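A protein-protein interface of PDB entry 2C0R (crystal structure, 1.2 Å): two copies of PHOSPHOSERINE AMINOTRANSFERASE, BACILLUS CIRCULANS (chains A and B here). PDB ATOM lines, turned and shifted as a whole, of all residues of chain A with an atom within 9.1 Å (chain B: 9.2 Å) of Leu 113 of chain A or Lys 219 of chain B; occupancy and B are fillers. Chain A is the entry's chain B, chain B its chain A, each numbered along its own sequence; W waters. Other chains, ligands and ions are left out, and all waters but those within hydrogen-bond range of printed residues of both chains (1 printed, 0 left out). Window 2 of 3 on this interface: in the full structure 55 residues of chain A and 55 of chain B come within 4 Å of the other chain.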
ATOM      1  N   SER A  78     -14.661   5.047  16.318  1.00  0.00           N
ATOM      2  CA  SER A  78     -14.715   3.700  16.862  1.00  0.00           C
ATOM      3  C   SER A  78     -13.585   2.805  16.334  1.00  0.00           C
ATOM      4  O   SER A  78     -13.118   1.916  17.033  1.00  0.00           O
ATOM      5  CB  SER A  78     -16.065   3.032  16.564  1.00  0.00           C
ATOM      6  OG  SER A  78     -17.088   3.798  17.198  1.00  0.00           O
ATOM      7  N   PHE A  81     -10.522   3.398  18.290  1.00  0.00           N
ATOM      8  CA  PHE A  81     -10.442   2.716  19.604  1.00  0.00           C
ATOM      9  C   PHE A  81      -9.641   1.429  19.532  1.00  0.00           C
ATOM     10  O   PHE A  81      -9.002   1.079  20.534  1.00  0.00           O
ATOM     11  CB  PHE A  81     -11.831   2.389  20.124  1.00  0.00           C
ATOM     12  CG  PHE A  81     -12.734   3.583  20.404  1.00  0.00           C
ATOM     13  CD1 PHE A  81     -14.099   3.361  20.500  1.00  0.00           C
ATOM     14  CD2 PHE A  81     -12.230   4.850  20.566  1.00  0.00           C
ATOM     15  CE1 PHE A  81     -14.965   4.383  20.784  1.00  0.00           C
ATOM     16  CE2 PHE A  81     -13.089   5.873  20.905  1.00  0.00           C
ATOM     17  CZ  PHE A  81     -14.440   5.661  20.993  1.00  0.00           C
ATOM     18  N   ALA A  82      -9.680   0.735  18.388  1.00  0.00           N
ATOM     19  CA  ALA A  82      -8.846  -0.472  18.222  1.00  0.00           C
ATOM     20  C   ALA A  82      -7.503  -0.118  17.611  1.00  0.00           C
ATOM     21  O   ALA A  82      -6.468  -0.701  17.995  1.00  0.00           O
ATOM     22  CB  ALA A  82      -9.574  -1.498  17.356  1.00  0.00           C
ATOM     23  N   PRO A  85      -4.589   1.059  20.347  1.00  0.00           N
ATOM     24  CA  PRO A  85      -3.820   0.022  21.031  1.00  0.00           C
ATOM     25  C   PRO A  85      -3.170  -0.951  20.060  1.00  0.00           C
ATOM     26  O   PRO A  85      -2.054  -1.428  20.368  1.00  0.00           O
ATOM     27  CB  PRO A  85      -4.871  -0.686  21.915  1.00  0.00           C
ATOM     28  CG  PRO A  85      -6.173  -0.360  21.260  1.00  0.00           C
ATOM     29  CD  PRO A  85      -6.009   1.037  20.727  1.00  0.00           C
ATOM     30  N   MET A  86      -3.791  -1.283  18.935  1.00  0.00           N
ATOM     31  CA  MET A  86      -3.070  -2.188  18.020  1.00  0.00           C
ATOM     32  C   MET A  86      -1.712  -1.653  17.650  1.00  0.00           C
ATOM     33  O   MET A  86      -0.752  -2.449  17.534  1.00  0.00           O
ATOM     34  CB  MET A  86      -3.929  -2.443  16.769  1.00  0.00           C
ATOM     35  CG  MET A  86      -5.129  -3.320  17.138  1.00  0.00           C
ATOM     36  SD  MET A  86      -6.274  -3.562  15.755  1.00  0.00           S
ATOM     37  CE  MET A  86      -5.975  -5.299  15.401  1.00  0.00           C
ATOM     38  N   LEU A  89       0.237  -0.528  21.805  1.00  0.00           N
ATOM     39  CA  LEU A  89       0.224  -1.365  23.010  1.00  0.00           C
ATOM     40  C   LEU A  89       1.018  -2.621  22.709  1.00  0.00           C
ATOM     41  O   LEU A  89       0.565  -3.488  21.951  1.00  0.00           O
ATOM     42  CB  LEU A  89      -1.210  -1.651  23.427  1.00  0.00           C
ATOM     43  CG  LEU A  89      -1.396  -2.442  24.727  1.00  0.00           C
ATOM     44  CD1 LEU A  89      -0.604  -1.836  25.876  1.00  0.00           C
ATOM     45  CD2 LEU A  89      -2.891  -2.527  25.019  1.00  0.00           C
ATOM     46  N   ALA A  95      -1.972   0.060  28.428  1.00  0.00           N
ATOM     47  CA  ALA A  95      -2.650   1.220  27.841  1.00  0.00           C
ATOM     48  C   ALA A  95      -3.393   1.920  28.961  1.00  0.00           C
ATOM     49  O   ALA A  95      -4.245   1.293  29.593  1.00  0.00           O
ATOM     50  CB  ALA A  95      -3.598   0.772  26.744  1.00  0.00           C
ATOM     51  N   TYR A  97      -5.964   4.716  30.556  1.00  0.00           N
ATOM     52  CA  TYR A  97      -7.183   5.431  30.192  1.00  0.00           C
ATOM     53  C   TYR A  97      -7.639   6.336  31.339  1.00  0.00           C
ATOM     54  O   TYR A  97      -7.606   5.928  32.495  1.00  0.00           O
ATOM     55  CB  TYR A  97      -8.354   4.491  29.769  1.00  0.00           C
ATOM     56  CG  TYR A  97      -8.013   3.947  28.388  1.00  0.00           C
ATOM     57  CD1 TYR A  97      -7.062   2.939  28.205  1.00  0.00           C
ATOM     58  CD2 TYR A  97      -8.667   4.509  27.280  1.00  0.00           C
ATOM     59  CE1 TYR A  97      -6.784   2.470  26.928  1.00  0.00           C
ATOM     60  CE2 TYR A  97      -8.349   4.049  26.025  1.00  0.00           C
ATOM     61  CZ  TYR A  97      -7.425   3.029  25.828  1.00  0.00           C
ATOM     62  OH  TYR A  97      -7.073   2.574  24.566  1.00  0.00           O
ATOM     63  N   LYS A 106     -16.144   3.111  26.036  1.00  0.00           N
ATOM     64  CA  LYS A 106     -16.018   2.397  24.740  1.00  0.00           C
ATOM     65  C   LYS A 106     -14.553   2.218  24.369  1.00  0.00           C
ATOM     66  O   LYS A 106     -14.124   1.158  23.875  1.00  0.00           O
ATOM     67  CB  LYS A 106     -16.710   3.153  23.603  1.00  0.00           C
ATOM     68  CG  LYS A 106     -18.238   3.126  23.674  1.00  0.00           C
ATOM     69  CD  LYS A 106     -18.768   1.857  23.069  1.00  0.00           C
ATOM     70  CE  LYS A 106     -20.227   1.883  22.649  1.00  0.00           C
ATOM     71  NZ  LYS A 106     -20.750   0.524  22.301  1.00  0.00           N
ATOM     72  N   ALA A 107     -13.744   3.266  24.564  1.00  0.00           N
ATOM     73  CA  ALA A 107     -12.338   3.217  24.151  1.00  0.00           C
ATOM     74  C   ALA A 107     -11.619   2.151  24.998  1.00  0.00           C
ATOM     75  O   ALA A 107     -10.865   1.321  24.481  1.00  0.00           O
ATOM     76  CB  ALA A 107     -11.689   4.561  24.252  1.00  0.00           C
ATOM     77  N   LEU A 108     -11.848   2.136  26.306  1.00  0.00           N
ATOM     78  CA  LEU A 108     -11.157   1.177  27.158  1.00  0.00           C
ATOM     79  C   LEU A 108     -11.556  -0.244  26.801  1.00  0.00           C
ATOM     80  O   LEU A 108     -10.699  -1.149  26.772  1.00  0.00           O
ATOM     81  CB  LEU A 108     -11.497   1.467  28.637  1.00  0.00           C
ATOM     82  CG  LEU A 108     -10.983   0.389  29.611  1.00  0.00           C
ATOM     83  CD1 LEU A 108      -9.466   0.388  29.649  1.00  0.00           C
ATOM     84  CD2 LEU A 108     -11.542   0.647  30.998  1.00  0.00           C
ATOM     85  N   LYS A 109     -12.849  -0.459  26.542  1.00  0.00           N
ATOM     86  CA  LYS A 109     -13.332  -1.816  26.236  1.00  0.00           C
ATOM     87  C   LYS A 109     -12.560  -2.365  25.047  1.00  0.00           C
ATOM     88  O   LYS A 109     -12.175  -3.534  25.031  1.00  0.00           O
ATOM     89  CB  LYS A 109     -14.842  -1.816  26.007  1.00  0.00           C
ATOM     90  CG  LYS A 109     -15.576  -3.128  25.985  1.00  0.00           C
ATOM     91  CD  LYS A 109     -17.088  -2.934  25.796  1.00  0.00           C
ATOM     92  CE  LYS A 109     -17.783  -4.252  25.504  1.00  0.00           C
ATOM     93  NZ  LYS A 109     -18.764  -4.672  26.564  1.00  0.00           N
ATOM     94  N   GLU A 110     -12.322  -1.549  24.023  1.00  0.00           N
ATOM     95  CA  GLU A 110     -11.595  -2.005  22.848  1.00  0.00           C
ATOM     96  C   GLU A 110     -10.153  -2.347  23.132  1.00  0.00           C
ATOM     97  O   GLU A 110      -9.626  -3.352  22.648  1.00  0.00           O
ATOM     98  CB  GLU A 110     -11.539  -0.866  21.790  1.00  0.00           C
ATOM     99  CG  GLU A 110     -12.746  -0.873  20.944  1.00  0.00           C
ATOM    100  CD  GLU A 110     -13.246  -2.210  20.424  1.00  0.00           C
ATOM    101  OE1 GLU A 110     -14.343  -2.554  20.921  1.00  0.00           O
ATOM    102  OE2 GLU A 110     -12.673  -2.939  19.577  1.00  0.00           O
ATOM    103  N   ALA A 111      -9.505  -1.489  23.957  1.00  0.00           N
ATOM    104  CA  ALA A 111      -8.107  -1.767  24.312  1.00  0.00           C
ATOM    105  C   ALA A 111      -7.897  -3.090  25.016  1.00  0.00           C
ATOM    106  O   ALA A 111      -6.892  -3.778  24.863  1.00  0.00           O
ATOM    107  CB  ALA A 111      -7.553  -0.604  25.142  1.00  0.00           C
ATOM    108  N   LYS A 112      -8.883  -3.453  25.844  1.00  0.00           N
ATOM    109  CA  LYS A 112      -8.779  -4.712  26.573  1.00  0.00           C
ATOM    110  C   LYS A 112      -8.733  -5.896  25.636  1.00  0.00           C
ATOM    111  O   LYS A 112      -8.213  -6.961  26.000  1.00  0.00           O
ATOM    112  CB  LYS A 112     -10.007  -4.789  27.500  1.00  0.00           C
ATOM    113  CG  LYS A 112      -9.855  -3.845  28.687  1.00  0.00           C
ATOM    114  CD  LYS A 112     -11.026  -4.125  29.646  1.00  0.00           C
ATOM    115  CE  LYS A 112     -10.827  -3.219  30.865  1.00  0.00           C
ATOM    116  NZ  LYS A 112     -11.994  -3.358  31.775  1.00  0.00           N
ATOM    117  N   LEU A 113      -9.262  -5.738  24.418  1.00  0.00           N
ATOM    118  CA  LEU A 113      -9.170  -6.873  23.500  1.00  0.00           C
ATOM    119  C   LEU A 113      -7.739  -7.063  22.996  1.00  0.00           C
ATOM    120  O   LEU A 113      -7.347  -8.131  22.518  1.00  0.00           O
ATOM    121  CB  LEU A 113     -10.062  -6.691  22.269  1.00  0.00           C
ATOM    122  CG  LEU A 113     -11.567  -6.556  22.506  1.00  0.00           C
ATOM    123  CD1 LEU A 113     -12.343  -5.926  21.346  1.00  0.00           C
ATOM    124  CD2 LEU A 113     -12.105  -7.935  22.862  1.00  0.00           C
ATOM    125  N   ILE A 114      -6.962  -5.979  23.065  1.00  0.00           N
ATOM    126  CA  ILE A 114      -5.628  -5.960  22.483  1.00  0.00           C
ATOM    127  C   ILE A 114      -4.545  -6.260  23.486  1.00  0.00           C
ATOM    128  O   ILE A 114      -3.544  -6.912  23.130  1.00  0.00           O
ATOM    129  CB  ILE A 114      -5.382  -4.585  21.830  1.00  0.00           C
ATOM    130  CG1 ILE A 114      -6.472  -4.208  20.813  1.00  0.00           C
ATOM    131  CG2 ILE A 114      -3.999  -4.523  21.188  1.00  0.00           C
ATOM    132  CD1 ILE A 114      -6.558  -5.345  19.799  1.00  0.00           C
ATOM    133  N   GLY A 115      -4.720  -5.742  24.705  1.00  0.00           N
ATOM    134  CA  GLY A 115      -3.690  -6.004  25.688  1.00  0.00           C
ATOM    135  C   GLY A 115      -4.030  -5.460  27.078  1.00  0.00           C
ATOM    136  O   GLY A 115      -5.183  -5.243  27.393  1.00  0.00           O
ATOM    137  N   ASP A 116      -2.974  -5.273  27.884  1.00  0.00           N
ATOM    138  CA  ASP A 116      -3.176  -4.882  29.276  1.00  0.00           C
ATOM    139  C   ASP A 116      -3.549  -3.396  29.337  1.00  0.00           C
ATOM    140  O   ASP A 116      -3.048  -2.598  28.566  1.00  0.00           O
ATOM    141  CB  ASP A 116      -1.896  -5.169  30.039  1.00  0.00           C
ATOM    142  CG  ASP A 116      -1.634  -6.657  30.146  1.00  0.00           C
ATOM    143  OD1 ASP A 116      -2.616  -7.435  30.082  1.00  0.00           O
ATOM    144  OD2 ASP A 116      -0.439  -7.038  30.283  1.00  0.00           O
ATOM    145  N   THR A 117      -4.439  -3.074  30.237  1.00  0.00           N
ATOM    146  CA  THR A 117      -4.953  -1.734  30.398  1.00  0.00           C
ATOM    147  C   THR A 117      -4.864  -1.302  31.870  1.00  0.00           C
ATOM    148  O   THR A 117      -4.746  -2.133  32.774  1.00  0.00           O
ATOM    149  CB  THR A 117      -6.399  -1.597  29.910  1.00  0.00           C
ATOM    150  OG1 THR A 117      -7.218  -2.461  30.696  1.00  0.00           O
ATOM    151  CG2 THR A 117      -6.600  -1.987  28.441  1.00  0.00           C
ATOM    152  N   MET B  86      -9.670 -12.366   8.791  1.00  0.00           N
ATOM    153  CA  MET B  86      -9.841 -12.214  10.254  1.00  0.00           C
ATOM    154  C   MET B  86     -11.108 -12.887  10.739  1.00  0.00           C
ATOM    155  O   MET B  86     -11.125 -13.443  11.855  1.00  0.00           O
ATOM    156  CB  MET B  86      -9.837 -10.719  10.616  1.00  0.00           C
ATOM    157  CG  MET B  86      -8.457 -10.097  10.525  1.00  0.00           C
ATOM    158  SD  MET B  86      -8.516  -8.281  10.716  1.00  0.00           S
ATOM    159  CE  MET B  86      -7.687  -8.195  12.312  1.00  0.00           C
ATOM    160  N   ASN B  87     -12.167 -12.807   9.953  1.00  0.00           N
ATOM    161  CA  ASN B  87     -13.437 -13.358  10.426  1.00  0.00           C
ATOM    162  C   ASN B  87     -13.554 -14.857  10.135  1.00  0.00           C
ATOM    163  O   ASN B  87     -14.238 -15.526  10.923  1.00  0.00           O
ATOM    164  CB  ASN B  87     -14.629 -12.628   9.804  1.00  0.00           C
ATOM    165  CG  ASN B  87     -14.954 -11.361  10.563  1.00  0.00           C
ATOM    166  OD1 ASN B  87     -15.886 -11.400  11.366  1.00  0.00           O
ATOM    167  ND2 ASN B  87     -14.190 -10.297  10.357  1.00  0.00           N
ATOM    168  N   ALA B 215     -23.037 -15.349  11.824  1.00  0.00           N
ATOM    169  CA  ALA B 215     -23.921 -15.283  12.981  1.00  0.00           C
ATOM    170  C   ALA B 215     -23.141 -15.011  14.260  1.00  0.00           C
ATOM    171  O   ALA B 215     -23.592 -14.340  15.195  1.00  0.00           O
ATOM    172  CB  ALA B 215     -24.719 -16.571  13.065  1.00  0.00           C
ATOM    173  N   GLU B 216     -21.931 -15.570  14.344  1.00  0.00           N
ATOM    174  CA  GLU B 216     -21.095 -15.334  15.527  1.00  0.00           C
ATOM    175  C   GLU B 216     -19.682 -15.055  15.024  1.00  0.00           C
ATOM    176  O   GLU B 216     -19.032 -15.989  14.514  1.00  0.00           O
ATOM    177  CB  GLU B 216     -21.097 -16.540  16.442  1.00  0.00           C
ATOM    178  CG  GLU B 216     -22.396 -17.236  16.787  1.00  0.00           C
ATOM    179  CD  GLU B 216     -22.203 -18.345  17.820  1.00  0.00           C
ATOM    180  OE1 GLU B 216     -22.831 -19.426  17.713  1.00  0.00           O
ATOM    181  OE2 GLU B 216     -21.387 -18.119  18.752  1.00  0.00           O
ATOM    182  N   SER B 217     -19.206 -13.844  15.115  1.00  0.00           N
ATOM    183  CA  SER B 217     -17.858 -13.503  14.660  1.00  0.00           C
ATOM    184  C   SER B 217     -16.811 -13.786  15.753  1.00  0.00           C
ATOM    185  O   SER B 217     -17.139 -13.808  16.947  1.00  0.00           O
ATOM    186  CB  SER B 217     -17.772 -12.044  14.263  1.00  0.00           C
ATOM    187  OG  SER B 217     -18.824 -11.726  13.309  1.00  0.00           O
ATOM    188  N   PRO B 218     -15.557 -14.005  15.378  1.00  0.00           N
ATOM    189  CA  PRO B 218     -14.537 -14.260  16.401  1.00  0.00           C
ATOM    190  C   PRO B 218     -14.445 -13.172  17.453  1.00  0.00           C
ATOM    191  O   PRO B 218     -14.334 -11.978  17.201  1.00  0.00           O
ATOM    192  CB  PRO B 218     -13.241 -14.279  15.579  1.00  0.00           C
ATOM    193  CG  PRO B 218     -13.721 -14.830  14.259  1.00  0.00           C
ATOM    194  CD  PRO B 218     -15.012 -14.104  13.996  1.00  0.00           C
ATOM    195  N   LYS B 219     -14.494 -13.632  18.717  1.00  0.00           N
ATOM    196  CA  LYS B 219     -14.590 -12.694  19.852  1.00  0.00           C
ATOM    197  C   LYS B 219     -13.308 -11.974  20.165  1.00  0.00           C
ATOM    198  O   LYS B 219     -13.295 -10.974  20.903  1.00  0.00           O
ATOM    199  CB  LYS B 219     -15.096 -13.521  21.045  1.00  0.00           C
ATOM    200  CG  LYS B 219     -16.603 -13.724  20.912  1.00  0.00           C
ATOM    201  CD  LYS B 219     -17.198 -14.402  22.135  1.00  0.00           C
ATOM    202  CE  LYS B 219     -18.591 -13.899  22.449  1.00  0.00           C
ATOM    203  NZ  LYS B 219     -18.716 -13.220  23.776  1.00  0.00           N
ATOM    204  N   HIS B 220     -12.173 -12.427  19.618  1.00  0.00           N
ATOM    205  CA  HIS B 220     -10.950 -11.672  19.900  1.00  0.00           C
ATOM    206  C   HIS B 220     -10.753 -10.462  19.011  1.00  0.00           C
ATOM    207  O   HIS B 220      -9.862  -9.661  19.246  1.00  0.00           O
ATOM    208  CB  HIS B 220      -9.755 -12.604  19.698  1.00  0.00           C
ATOM    209  CG  HIS B 220      -9.675 -13.143  18.310  1.00  0.00           C
ATOM    210  ND1 HIS B 220     -10.309 -14.312  17.944  1.00  0.00           N
ATOM    211  CD2 HIS B 220      -9.042 -12.684  17.200  1.00  0.00           C
ATOM    212  CE1 HIS B 220     -10.081 -14.569  16.669  1.00  0.00           C
ATOM    213  NE2 HIS B 220      -9.323 -13.601  16.207  1.00  0.00           N
ATOM    214  N   LEU B 221     -11.567 -10.310  17.973  1.00  0.00           N
ATOM    215  CA  LEU B 221     -11.415  -9.284  16.971  1.00  0.00           C
ATOM    216  C   LEU B 221     -11.869  -7.906  17.451  1.00  0.00           C
ATOM    217  O   LEU B 221     -12.844  -7.872  18.203  1.00  0.00           O
ATOM    218  CB  LEU B 221     -12.299  -9.598  15.749  1.00  0.00           C
ATOM    219  CG  LEU B 221     -11.764 -10.760  14.893  1.00  0.00           C
ATOM    220  CD1 LEU B 221     -12.721 -11.003  13.734  1.00  0.00           C
ATOM    221  CD2 LEU B 221     -10.360 -10.519  14.377  1.00  0.00           C
ATOM    222  N   PRO B 222     -11.259  -6.836  16.943  1.00  0.00           N
ATOM    223  CA  PRO B 222     -11.753  -5.478  17.172  1.00  0.00           C
ATOM    224  C   PRO B 222     -13.239  -5.488  16.775  1.00  0.00           C
ATOM    225  O   PRO B 222     -13.631  -6.107  15.800  1.00  0.00           O
ATOM    226  CB  PRO B 222     -10.910  -4.596  16.254  1.00  0.00           C
ATOM    227  CG  PRO B 222      -9.654  -5.403  16.026  1.00  0.00           C
ATOM    228  CD  PRO B 222     -10.076  -6.844  16.036  1.00  0.00           C
ATOM    229  N   THR B 223     -14.027  -4.782  17.580  1.00  0.00           N
ATOM    230  CA  THR B 223     -15.462  -4.679  17.335  1.00  0.00           C
ATOM    231  C   THR B 223     -15.754  -4.296  15.900  1.00  0.00           C
ATOM    232  O   THR B 223     -16.631  -4.847  15.247  1.00  0.00           O
ATOM    233  CB  THR B 223     -16.105  -3.651  18.309  1.00  0.00           C
ATOM    234  OG1 THR B 223     -15.811  -4.093  19.638  1.00  0.00           O
ATOM    235  CG2 THR B 223     -17.621  -3.581  18.118  1.00  0.00           C
ATOM    236  N   MET B 224     -15.035  -3.273  15.462  1.00  0.00           N
ATOM    237  CA  MET B 224     -15.320  -2.755  14.113  1.00  0.00           C
ATOM    238  C   MET B 224     -14.845  -3.703  13.021  1.00  0.00           C
ATOM    239  O   MET B 224     -15.104  -3.416  11.855  1.00  0.00           O
ATOM    240  CB  MET B 224     -14.641  -1.380  13.981  1.00  0.00           C
ATOM    241  CG  MET B 224     -15.333  -0.353  14.869  1.00  0.00           C
ATOM    242  SD  MET B 224     -17.053  -0.089  14.473  1.00  0.00           S
ATOM    243  CE  MET B 224     -16.873   0.588  12.803  1.00  0.00           C
ATOM    244  N   LEU B 225     -14.150  -4.773  13.369  1.00  0.00           N
ATOM    245  CA  LEU B 225     -13.698  -5.714  12.353  1.00  0.00           C
ATOM    246  C   LEU B 225     -14.415  -7.046  12.454  1.00  0.00           C
ATOM    247  O   LEU B 225     -13.978  -8.020  11.840  1.00  0.00           O
ATOM    248  CB  LEU B 225     -12.182  -5.897  12.434  1.00  0.00           C
ATOM    249  CG  LEU B 225     -11.485  -4.744  11.684  1.00  0.00           C
ATOM    250  CD1 LEU B 225     -10.016  -4.825  12.078  1.00  0.00           C
ATOM    251  CD2 LEU B 225     -11.696  -4.815  10.183  1.00  0.00           C
ATOM    252  N   ARG B 226     -15.525  -7.075  13.171  1.00  0.00           N
ATOM    253  CA  ARG B 226     -16.370  -8.258  13.227  1.00  0.00           C
ATOM    254  C   ARG B 226     -17.551  -8.071  12.300  1.00  0.00           C
ATOM    255  O   ARG B 226     -18.205  -7.009  12.377  1.00  0.00           O
ATOM    256  CB  ARG B 226     -16.921  -8.473  14.650  1.00  0.00           C
ATOM    257  CG  ARG B 226     -15.851  -9.007  15.592  1.00  0.00           C
ATOM    258  CD  ARG B 226     -16.331  -8.925  17.045  1.00  0.00           C
ATOM    259  NE  ARG B 226     -17.508  -9.766  17.264  1.00  0.00           N
ATOM    260  CZ  ARG B 226     -17.865 -10.272  18.445  1.00  0.00           C
ATOM    261  NH1 ARG B 226     -17.173 -10.085  19.561  1.00  0.00           N
ATOM    262  NH2 ARG B 226     -18.971 -11.011  18.447  1.00  0.00           N
ATOM    263  N   ASP B 228     -20.442  -9.537  12.598  1.00  0.00           N
ATOM    264  CA  ASP B 228     -21.725  -9.486  13.351  1.00  0.00           C
ATOM    265  C   ASP B 228     -21.969  -8.114  13.941  1.00  0.00           C
ATOM    266  O   ASP B 228     -23.134  -7.728  14.187  1.00  0.00           O
ATOM    267  CB  ASP B 228     -21.716 -10.621  14.382  1.00  0.00           C
ATOM    268  CG  ASP B 228     -20.651 -10.570  15.454  1.00  0.00           C
ATOM    269  OD1 ASP B 228     -19.850  -9.623  15.561  1.00  0.00           O
ATOM    270  OD2 ASP B 228     -20.597 -11.562  16.228  1.00  0.00           O
ATOM    271  N   THR B 229     -20.921  -7.324  14.151  1.00  0.00           N
ATOM    272  CA  THR B 229     -21.177  -5.913  14.561  1.00  0.00           C
ATOM    273  C   THR B 229     -22.061  -5.206  13.554  1.00  0.00           C
ATOM    274  O   THR B 229     -22.915  -4.393  13.903  1.00  0.00           O
ATOM    275  CB  THR B 229     -19.848  -5.146  14.670  1.00  0.00           C
ATOM    276  OG1 THR B 229     -19.121  -5.811  15.702  1.00  0.00           O
ATOM    277  CG2 THR B 229     -20.074  -3.657  14.994  1.00  0.00           C
ATOM    278  N   LYS B 232     -25.731  -7.288  13.306  1.00  0.00           N
ATOM    279  CA  LYS B 232     -26.613  -7.140  14.458  1.00  0.00           C
ATOM    280  C   LYS B 232     -27.079  -5.711  14.618  1.00  0.00           C
ATOM    281  O   LYS B 232     -28.110  -5.484  15.219  1.00  0.00           O
ATOM    282  CB  LYS B 232     -25.866  -7.598  15.729  1.00  0.00           C
ATOM    283  CG  LYS B 232     -25.614  -9.113  15.649  1.00  0.00           C
ATOM    284  CD  LYS B 232     -24.882  -9.616  16.894  1.00  0.00           C
ATOM    285  CE  LYS B 232     -25.178 -11.127  17.036  1.00  0.00           C
ATOM    286  NZ  LYS B 232     -25.684 -11.566  15.673  1.00  0.00           N
ATOM    287  N   TYR B 237     -23.852   0.445  14.090  1.00  0.00           N
ATOM    288  CA  TYR B 237     -23.202   0.390  15.382  1.00  0.00           C
ATOM    289  C   TYR B 237     -22.489   1.689  15.687  1.00  0.00           C
ATOM    290  O   TYR B 237     -22.557   2.183  16.804  1.00  0.00           O
ATOM    291  CB  TYR B 237     -22.212  -0.809  15.415  1.00  0.00           C
ATOM    292  CG  TYR B 237     -21.406  -0.768  16.716  1.00  0.00           C
ATOM    293  CD1 TYR B 237     -21.928  -1.219  17.930  1.00  0.00           C
ATOM    294  CD2 TYR B 237     -20.098  -0.287  16.704  1.00  0.00           C
ATOM    295  CE1 TYR B 237     -21.154  -1.154  19.085  1.00  0.00           C
ATOM    296  CE2 TYR B 237     -19.341  -0.211  17.843  1.00  0.00           C
ATOM    297  CZ  TYR B 237     -19.878  -0.646  19.035  1.00  0.00           C
ATOM    298  OH  TYR B 237     -19.071  -0.586  20.167  1.00  0.00           O
HETATM  299  O   HOH W   1     -13.054  -1.830  16.952  1.00  0.00           O
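Among the printed residues, pairs that only touch across the chains: Ser 78 of chain A with Met 224 of chain B (3.8 Å), Ala 82 of chain A with Pro 222 of chain B (3.5 Å), Met 86 of chain A with Pro 222 of chain B (3.7 Å), Glu 110 of chain A with Pro 222 of chain B (3.6 Å), Leu 113 of chain A with Lys 219 of chain B (3.8 Å) and Leu 113 of chain A with Leu 221 of chain B (3.7 Å).
Of chain B, only Lys 219 and Leu 221 come within 4 Å of Leu 113 of chain A.
Glu 110 of chain A touches just these residues of chain B: Pro 222 (3.6 Å) and Thr 223 (2.5 Å).
No residue of chain A comes within 4 Å of Pro 218 of chain B.
Of the printed residues of chain A, Thr 223 of chain B touches Glu 110 (2.5 Å).
Printed residues of chain B within 4 Å of Lys 106 of chain A: Tyr 237.
Of the printed residues of chain A, Pro 222 of chain B touches Ala 82 (3.5 Å), Met 86 (3.7 Å) and Glu 110 (3.6 Å).
Of the printed residues of chain B, Ser 78 of chain A touches Met 224 (3.8 Å).
The nearest printed residue of chain B that does not touch Leu 113 of chain A is Pro 222 of chain B (4.2 Å).
The nearest printed residue of chain A that does not touch Tyr 237 of chain B is Ser 78 of chain A (4.6 Å).
The backbone carbonyl oxygen of Thr 223 of chain B sits at hydrogen-bond distance from the side-chain hydroxyl of Thr 229 of chain B (2.7 Å).
Printed residues of chain B that touch a printed residue of chain A: Lys 219, Leu 221, Pro 222, Thr 223, Met 224 and Tyr 237.
Hydrophobic or aromatic side chains of chain B within 4 Å of the printed part of chain A: Pro 222, Met 224 and Tyr 237.
1 position is printed for both chains.
Of the 8 pairs that touch across the chains among the printed residues, none has its exchanged pair printed and touching as well.
The side-chain hydroxyl (OG1) of Thr 223 of chain B sits at hydrogen-bond distance from the side-chain carboxylate (OE1) of Glu 110 of chain A (2.5 Å).
The side-chain hydroxyl (OH) of Tyr 237 of chain B sits at hydrogen-bond distance from the side-chain amino group (NZ) of Lys 106 of chain A (2.9 Å).
Water W1 lies within hydrogen-bond range of N of Met 224 of chain B (2.9 Å), OE2 of Glu 110 of chain A (2.9 Å) and N of Thr 223 of chain B (3.2 Å).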
